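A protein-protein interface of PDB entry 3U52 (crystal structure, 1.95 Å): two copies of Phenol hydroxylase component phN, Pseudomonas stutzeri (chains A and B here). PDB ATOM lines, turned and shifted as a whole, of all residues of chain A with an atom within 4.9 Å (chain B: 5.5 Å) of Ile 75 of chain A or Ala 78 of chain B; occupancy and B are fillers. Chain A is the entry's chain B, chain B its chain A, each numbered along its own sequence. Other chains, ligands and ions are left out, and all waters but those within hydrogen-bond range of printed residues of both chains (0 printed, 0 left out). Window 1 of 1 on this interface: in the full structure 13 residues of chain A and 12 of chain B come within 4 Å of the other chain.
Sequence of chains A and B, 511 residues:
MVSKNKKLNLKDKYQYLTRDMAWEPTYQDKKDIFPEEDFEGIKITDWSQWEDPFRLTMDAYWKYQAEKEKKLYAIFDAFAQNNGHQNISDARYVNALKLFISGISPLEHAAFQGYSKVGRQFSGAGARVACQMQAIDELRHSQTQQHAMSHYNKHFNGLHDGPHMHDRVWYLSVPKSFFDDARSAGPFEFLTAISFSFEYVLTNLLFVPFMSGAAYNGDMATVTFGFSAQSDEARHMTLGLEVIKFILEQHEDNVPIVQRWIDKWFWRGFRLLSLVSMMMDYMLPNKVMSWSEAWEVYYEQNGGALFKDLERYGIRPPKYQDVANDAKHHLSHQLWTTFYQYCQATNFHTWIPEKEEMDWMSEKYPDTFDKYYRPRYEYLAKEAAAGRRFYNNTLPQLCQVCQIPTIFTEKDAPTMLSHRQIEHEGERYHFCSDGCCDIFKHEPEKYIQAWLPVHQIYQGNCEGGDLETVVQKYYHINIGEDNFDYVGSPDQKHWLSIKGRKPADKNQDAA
The side-chain amide nitrogen of Asn 82 of chain B lies within hydrogen-bond range of the backbone carbonyl oxygen of Ala 78 of chain B, at 2.8 Å.
ND2 of Asn 82 of chain B lies close to NE2 of Gln 81 of chain B (3.1 Å).
O of Met 220 of chain A is in hydrogen-bond range of OG1 of Thr 224 of chain A (2.6 Å).
Lys 71 of chain A touches Ala 74 of chain B.
Ile 75 of chain B touches Ala 74 of chain A.
Ile 75 of chain A touches Ala 74 of chain B.
Ile 75 of chain A touches Ala 78 of chain B.
Ala 78 of chain A touches Ile 75 of chain B.
Ala 78 of chain B touches Met 220 of chain A.
CG of Met 220 of chain A touches ND2 of Asn 82 of chain B, 3.6 Å away.
Gln 81 of chain B touches Thr 224 of chain A.
Of the printed residues of chain B, Lys 71 of chain A touches Ala 74 (3.8 Å).
Tyr 73 of chain A touches none of the printed residues of chain B.
Of chain B, only Ala 74 (3.4 Å) and Ala 78 (3.9 Å) come within 4 Å of Ile 75 of chain A.
Phe 76 of chain A touches none of the printed residues of chain B.
Of the printed residues of chain B, Thr 224 of chain A touches Gln 81 (3.7 Å).
Of chain A, only Ile 75 (3.9 Å) and Met 220 (3.7 Å) come within 4 Å of Ala 78 of chain B.
Of the printed residues of chain A, Gln 81 of chain B touches Thr 224.
The nearest residue of chain B that does not touch Ile 75 of chain A is Ile 75 of chain B (4.3 Å).
The nearest printed residue of chain B that does not touch Ala 78 of chain A is Ala 78 of chain B (7.1 Å).
Hydrophobic or aromatic side chains of chain B that line the printed part of chain A: Ala 74, Ile 75 and Ala 78.
Of the 11 printed residues of chain A, 6 touch a printed residue of chain B.
Printed residues of chain A that touch a printed residue of chain B: Lys 71, Ala 74, Ile 75, Ala 78, Met 220 and Thr 224.
Hydrophobic or aromatic side chains of chain A within 4 Å of the printed part of chain B: Ile 75, Ala 78 and Met 220.
Among the printed residues, 8 pairs touch across the chains.
Ala 74 of chain A touches Ile 75 of chain B, and with the chains exchanged Ile 75 of chain A touches Ala 74 of chain B.
Ile 75 of chain A touches Ala 78 of chain B, and with the chains exchanged Ala 78 of chain A touches Ile 75 of chain B.
Positions printed for both chains: 73, 74, 75, 76, 77, 78 and 79.
Of the 8 pairs that touch across the chains among the printed residues, 4 have their exchanged pair printed and touching as well.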
ATOM      1  N   LYS A  71     -25.169   5.948   6.716  1.00  0.00           N
ATOM      2  CA  LYS A  71     -26.021   5.845   5.547  1.00  0.00           C
ATOM      3  C   LYS A  71     -25.973   7.076   4.658  1.00  0.00           C
ATOM      4  O   LYS A  71     -25.780   6.959   3.449  1.00  0.00           O
ATOM      5  CB  LYS A  71     -27.458   5.574   5.991  1.00  0.00           C
ATOM      6  CG  LYS A  71     -27.596   4.182   6.670  1.00  0.00           C
ATOM      7  CD  LYS A  71     -29.041   3.745   6.814  1.00  0.00           C
ATOM      8  CE  LYS A  71     -29.803   4.443   7.904  1.00  0.00           C
ATOM      9  NZ  LYS A  71     -30.508   3.398   8.722  1.00  0.00           N
ATOM     10  N   LEU A  72     -26.137   8.253   5.261  1.00  0.00           N
ATOM     11  CA  LEU A  72     -26.023   9.526   4.533  1.00  0.00           C
ATOM     12  C   LEU A  72     -24.736   9.685   3.728  1.00  0.00           C
ATOM     13  O   LEU A  72     -24.789  10.015   2.517  1.00  0.00           O
ATOM     14  CB  LEU A  72     -26.188  10.712   5.496  1.00  0.00           C
ATOM     15  CG  LEU A  72     -26.180  12.110   4.860  1.00  0.00           C
ATOM     16  CD1 LEU A  72     -27.451  12.365   4.158  1.00  0.00           C
ATOM     17  CD2 LEU A  72     -25.983  13.155   5.969  1.00  0.00           C
ATOM     18  N   TYR A  73     -23.585   9.477   4.366  1.00  0.00           N
ATOM     19  CA  TYR A  73     -22.302   9.573   3.687  1.00  0.00           C
ATOM     20  C   TYR A  73     -22.076   8.483   2.627  1.00  0.00           C
ATOM     21  O   TYR A  73     -21.380   8.743   1.639  1.00  0.00           O
ATOM     22  CB  TYR A  73     -21.132   9.704   4.658  1.00  0.00           C
ATOM     23  CG  TYR A  73     -21.091  11.136   5.224  1.00  0.00           C
ATOM     24  CD1 TYR A  73     -20.586  12.193   4.472  1.00  0.00           C
ATOM     25  CD2 TYR A  73     -21.643  11.430   6.467  1.00  0.00           C
ATOM     26  CE1 TYR A  73     -20.592  13.534   4.980  1.00  0.00           C
ATOM     27  CE2 TYR A  73     -21.660  12.784   7.001  1.00  0.00           C
ATOM     28  CZ  TYR A  73     -21.120  13.811   6.246  1.00  0.00           C
ATOM     29  OH  TYR A  73     -21.124  15.113   6.733  1.00  0.00           O
ATOM     30  N   ALA A  74     -22.722   7.326   2.778  1.00  0.00           N
ATOM     31  CA  ALA A  74     -22.584   6.223   1.791  1.00  0.00           C
ATOM     32  C   ALA A  74     -23.332   6.636   0.497  1.00  0.00           C
ATOM     33  O   ALA A  74     -22.814   6.511  -0.600  1.00  0.00           O
ATOM     34  CB  ALA A  74     -23.177   4.963   2.351  1.00  0.00           C
ATOM     35  N   ILE A  75     -24.533   7.185   0.665  1.00  0.00           N
ATOM     36  CA  ILE A  75     -25.293   7.814  -0.429  1.00  0.00           C
ATOM     37  C   ILE A  75     -24.577   9.013  -1.086  1.00  0.00           C
ATOM     38  O   ILE A  75     -24.487   9.050  -2.315  1.00  0.00           O
ATOM     39  CB  ILE A  75     -26.723   8.106   0.034  1.00  0.00           C
ATOM     40  CG1 ILE A  75     -27.313   6.815   0.577  1.00  0.00           C
ATOM     41  CG2 ILE A  75     -27.625   8.744  -1.117  1.00  0.00           C
ATOM     42  CD1 ILE A  75     -28.531   6.955   1.496  1.00  0.00           C
ATOM     43  N   PHE A  76     -24.037   9.961  -0.295  1.00  0.00           N
ATOM     44  CA  PHE A  76     -23.253  11.084  -0.851  1.00  0.00           C
ATOM     45  C   PHE A  76     -22.128  10.569  -1.756  1.00  0.00           C
ATOM     46  O   PHE A  76     -21.953  11.059  -2.860  1.00  0.00           O
ATOM     47  CB  PHE A  76     -22.625  11.970   0.247  1.00  0.00           C
ATOM     48  CG  PHE A  76     -23.605  12.887   0.947  1.00  0.00           C
ATOM     49  CD1 PHE A  76     -24.928  13.007   0.517  1.00  0.00           C
ATOM     50  CD2 PHE A  76     -23.201  13.636   2.055  1.00  0.00           C
ATOM     51  CE1 PHE A  76     -25.825  13.878   1.176  1.00  0.00           C
ATOM     52  CE2 PHE A  76     -24.095  14.471   2.725  1.00  0.00           C
ATOM     53  CZ  PHE A  76     -25.411  14.590   2.286  1.00  0.00           C
ATOM     54  N   ASP A  77     -21.354   9.606  -1.251  1.00  0.00           N
ATOM     55  CA  ASP A  77     -20.270   9.015  -2.006  1.00  0.00           C
ATOM     56  C   ASP A  77     -20.747   8.350  -3.305  1.00  0.00           C
ATOM     57  O   ASP A  77     -20.157   8.576  -4.348  1.00  0.00           O
ATOM     58  CB  ASP A  77     -19.467   8.059  -1.122  1.00  0.00           C
ATOM     59  CG  ASP A  77     -18.587   8.812  -0.092  1.00  0.00           C
ATOM     60  OD1 ASP A  77     -18.046   8.168   0.867  1.00  0.00           O
ATOM     61  OD2 ASP A  77     -18.424  10.058  -0.244  1.00  0.00           O
ATOM     62  N   ALA A  78     -21.837   7.594  -3.233  1.00  0.00           N
ATOM     63  CA  ALA A  78     -22.415   6.936  -4.383  1.00  0.00           C
ATOM     64  C   ALA A  78     -22.927   7.941  -5.431  1.00  0.00           C
ATOM     65  O   ALA A  78     -22.677   7.764  -6.616  1.00  0.00           O
ATOM     66  CB  ALA A  78     -23.519   6.013  -3.936  1.00  0.00           C
ATOM     67  N   PHE A  79     -23.610   8.996  -4.982  1.00  0.00           N
ATOM     68  CA  PHE A  79     -24.081  10.103  -5.856  1.00  0.00           C
ATOM     69  C   PHE A  79     -22.930  10.668  -6.660  1.00  0.00           C
ATOM     70  O   PHE A  79     -23.028  10.780  -7.882  1.00  0.00           O
ATOM     71  CB  PHE A  79     -24.743  11.208  -5.001  1.00  0.00           C
ATOM     72  CG  PHE A  79     -25.299  12.378  -5.789  1.00  0.00           C
ATOM     73  CD1 PHE A  79     -26.524  12.284  -6.432  1.00  0.00           C
ATOM     74  CD2 PHE A  79     -24.616  13.587  -5.830  1.00  0.00           C
ATOM     75  CE1 PHE A  79     -27.047  13.390  -7.142  1.00  0.00           C
ATOM     76  CE2 PHE A  79     -25.131  14.690  -6.523  1.00  0.00           C
ATOM     77  CZ  PHE A  79     -26.340  14.578  -7.173  1.00  0.00           C
ATOM     78  N   MET A 220     -30.707  13.555  -5.699  1.00  0.00           N
ATOM     79  CA  MET A 220     -30.669  12.515  -4.673  1.00  0.00           C
ATOM     80  C   MET A 220     -29.950  12.969  -3.391  1.00  0.00           C
ATOM     81  O   MET A 220     -30.303  12.525  -2.287  1.00  0.00           O
ATOM     82  CB  MET A 220     -29.998  11.241  -5.227  1.00  0.00           C
ATOM     83  CG  MET A 220     -29.713  10.126  -4.167  1.00  0.00           C
ATOM     84  SD  MET A 220     -28.760   8.668  -4.796  1.00  0.00           S
ATOM     85  CE  MET A 220     -30.020   8.029  -5.914  1.00  0.00           C
ATOM     86  N   THR A 224     -31.773  13.120   0.178  1.00  0.00           N
ATOM     87  CA  THR A 224     -31.203  12.279   1.230  1.00  0.00           C
ATOM     88  C   THR A 224     -30.886  13.094   2.492  1.00  0.00           C
ATOM     89  O   THR A 224     -31.171  12.638   3.612  1.00  0.00           O
ATOM     90  CB  THR A 224     -29.985  11.456   0.742  1.00  0.00           C
ATOM     91  OG1 THR A 224     -30.400  10.678  -0.402  1.00  0.00           O
ATOM     92  CG2 THR A 224     -29.525  10.485   1.841  1.00  0.00           C
ATOM     93  N   TYR B  73     -26.686  -1.418   1.511  1.00  0.00           N
ATOM     94  CA  TYR B  73     -28.122  -1.308   1.688  1.00  0.00           C
ATOM     95  C   TYR B  73     -28.679   0.123   1.752  1.00  0.00           C
ATOM     96  O   TYR B  73     -29.770   0.384   1.261  1.00  0.00           O
ATOM     97  CB  TYR B  73     -28.607  -2.144   2.885  1.00  0.00           C
ATOM     98  CG  TYR B  73     -28.664  -3.596   2.456  1.00  0.00           C
ATOM     99  CD1 TYR B  73     -29.775  -4.098   1.755  1.00  0.00           C
ATOM    100  CD2 TYR B  73     -27.558  -4.425   2.631  1.00  0.00           C
ATOM    101  CE1 TYR B  73     -29.791  -5.446   1.320  1.00  0.00           C
ATOM    102  CE2 TYR B  73     -27.570  -5.762   2.200  1.00  0.00           C
ATOM    103  CZ  TYR B  73     -28.682  -6.261   1.548  1.00  0.00           C
ATOM    104  OH  TYR B  73     -28.708  -7.582   1.109  1.00  0.00           O
ATOM    105  N   ALA B  74     -27.891   1.032   2.301  1.00  0.00           N
ATOM    106  CA  ALA B  74     -28.239   2.481   2.299  1.00  0.00           C
ATOM    107  C   ALA B  74     -28.351   2.968   0.862  1.00  0.00           C
ATOM    108  O   ALA B  74     -29.258   3.726   0.534  1.00  0.00           O
ATOM    109  CB  ALA B  74     -27.173   3.276   3.004  1.00  0.00           C
ATOM    110  N   ILE B  75     -27.399   2.542   0.029  1.00  0.00           N
ATOM    111  CA  ILE B  75     -27.377   2.930  -1.388  1.00  0.00           C
ATOM    112  C   ILE B  75     -28.553   2.277  -2.123  1.00  0.00           C
ATOM    113  O   ILE B  75     -29.228   2.939  -2.946  1.00  0.00           O
ATOM    114  CB  ILE B  75     -26.010   2.602  -2.044  1.00  0.00           C
ATOM    115  CG1 ILE B  75     -24.931   3.520  -1.457  1.00  0.00           C
ATOM    116  CG2 ILE B  75     -26.047   2.765  -3.576  1.00  0.00           C
ATOM    117  CD1 ILE B  75     -23.482   3.109  -1.638  1.00  0.00           C
ATOM    118  N   PHE B  76     -28.797   0.986  -1.852  1.00  0.00           N
ATOM    119  CA  PHE B  76     -29.911   0.273  -2.500  1.00  0.00           C
ATOM    120  C   PHE B  76     -31.270   0.940  -2.203  1.00  0.00           C
ATOM    121  O   PHE B  76     -32.168   0.966  -3.089  1.00  0.00           O
ATOM    122  CB  PHE B  76     -30.014  -1.200  -2.033  1.00  0.00           C
ATOM    123  CG  PHE B  76     -29.008  -2.131  -2.645  1.00  0.00           C
ATOM    124  CD1 PHE B  76     -28.223  -1.761  -3.723  1.00  0.00           C
ATOM    125  CD2 PHE B  76     -28.904  -3.432  -2.159  1.00  0.00           C
ATOM    126  CE1 PHE B  76     -27.290  -2.670  -4.290  1.00  0.00           C
ATOM    127  CE2 PHE B  76     -27.961  -4.348  -2.695  1.00  0.00           C
ATOM    128  CZ  PHE B  76     -27.183  -3.978  -3.779  1.00  0.00           C
ATOM    129  N   ASP B  77     -31.489   1.353  -0.948  1.00  0.00           N
ATOM    130  CA  ASP B  77     -32.723   2.020  -0.573  1.00  0.00           C
ATOM    131  C   ASP B  77     -32.858   3.385  -1.250  1.00  0.00           C
ATOM    132  O   ASP B  77     -33.970   3.768  -1.593  1.00  0.00           O
ATOM    133  CB  ASP B  77     -32.842   2.255   0.944  1.00  0.00           C
ATOM    134  CG  ASP B  77     -32.928   0.974   1.758  1.00  0.00           C
ATOM    135  OD1 ASP B  77     -32.416   1.018   2.897  1.00  0.00           O
ATOM    136  OD2 ASP B  77     -33.510  -0.053   1.303  1.00  0.00           O
ATOM    137  N   ALA B  78     -31.755   4.123  -1.378  1.00  0.00           N
ATOM    138  CA  ALA B  78     -31.729   5.442  -2.010  1.00  0.00           C
ATOM    139  C   ALA B  78     -32.044   5.333  -3.514  1.00  0.00           C
ATOM    140  O   ALA B  78     -32.721   6.221  -4.107  1.00  0.00           O
ATOM    141  CB  ALA B  78     -30.346   6.076  -1.852  1.00  0.00           C
ATOM    142  N   PHE B  79     -31.490   4.289  -4.118  1.00  0.00           N
ATOM    143  CA  PHE B  79     -31.720   3.964  -5.529  1.00  0.00           C
ATOM    144  C   PHE B  79     -33.196   3.766  -5.788  1.00  0.00           C
ATOM    145  O   PHE B  79     -33.752   4.387  -6.708  1.00  0.00           O
ATOM    146  CB  PHE B  79     -30.900   2.720  -5.913  1.00  0.00           C
ATOM    147  CG  PHE B  79     -31.087   2.270  -7.331  1.00  0.00           C
ATOM    148  CD1 PHE B  79     -30.344   2.821  -8.345  1.00  0.00           C
ATOM    149  CD2 PHE B  79     -32.005   1.258  -7.635  1.00  0.00           C
ATOM    150  CE1 PHE B  79     -30.515   2.387  -9.692  1.00  0.00           C
ATOM    151  CE2 PHE B  79     -32.174   0.830  -8.954  1.00  0.00           C
ATOM    152  CZ  PHE B  79     -31.428   1.399  -9.966  1.00  0.00           C
ATOM    153  N   ALA B  80     -33.837   2.934  -4.963  1.00  0.00           N
ATOM    154  CA  ALA B  80     -35.250   2.612  -5.061  1.00  0.00           C
ATOM    155  C   ALA B  80     -36.165   3.808  -4.748  1.00  0.00           C
ATOM    156  O   ALA B  80     -37.144   4.031  -5.482  1.00  0.00           O
ATOM    157  CB  ALA B  80     -35.596   1.427  -4.130  1.00  0.00           C
ATOM    158  N   GLN B  81     -35.858   4.527  -3.654  1.00  0.00           N
ATOM    159  CA  GLN B  81     -36.626   5.697  -3.227  1.00  0.00           C
ATOM    160  C   GLN B  81     -36.582   6.803  -4.304  1.00  0.00           C
ATOM    161  O   GLN B  81     -37.598   7.477  -4.527  1.00  0.00           O
ATOM    162  CB  GLN B  81     -36.270   6.167  -1.778  1.00  0.00           C
ATOM    163  CG  GLN B  81     -35.535   7.534  -1.554  1.00  0.00           C
ATOM    164  CD  GLN B  81     -34.395   7.518  -0.409  1.00  0.00           C
ATOM    165  OE1 GLN B  81     -34.444   6.706   0.557  1.00  0.00           O
ATOM    166  NE2 GLN B  81     -33.370   8.439  -0.548  1.00  0.00           N
ATOM    167  N   ASN B  82     -35.448   6.922  -5.003  1.00  0.00           N
ATOM    168  CA  ASN B  82     -35.256   7.919  -6.059  1.00  0.00           C
ATOM    169  C   ASN B  82     -35.481   7.442  -7.502  1.00  0.00           C
ATOM    170  O   ASN B  82     -35.084   8.120  -8.461  1.00  0.00           O
ATOM    171  CB  ASN B  82     -33.917   8.633  -5.877  1.00  0.00           C
ATOM    172  CG  ASN B  82     -33.880   9.417  -4.551  1.00  0.00           C
ATOM    173  OD1 ASN B  82     -34.607  10.403  -4.389  1.00  0.00           O
ATOM    174  ND2 ASN B  82     -33.103   8.925  -3.580  1.00  0.00           N
ATOM    175  N   ASN B  83     -36.150   6.296  -7.650  1.00  0.00           N
ATOM    176  CA  ASN B  83     -36.407   5.684  -8.953  1.00  0.00           C
ATOM    177  C   ASN B  83     -35.216   5.732  -9.866  1.00  0.00           C
ATOM    178  O   ASN B  83     -35.260   6.267 -10.971  1.00  0.00           O
ATOM    179  CB  ASN B  83     -37.635   6.310  -9.590  1.00  0.00           C
ATOM    180  CG  ASN B  83     -38.897   5.907  -8.884  1.00  0.00           C
ATOM    181  OD1 ASN B  83     -39.204   4.701  -8.709  1.00  0.00           O
ATOM    182  ND2 ASN B  83     -39.632   6.905  -8.435  1.00  0.00           N
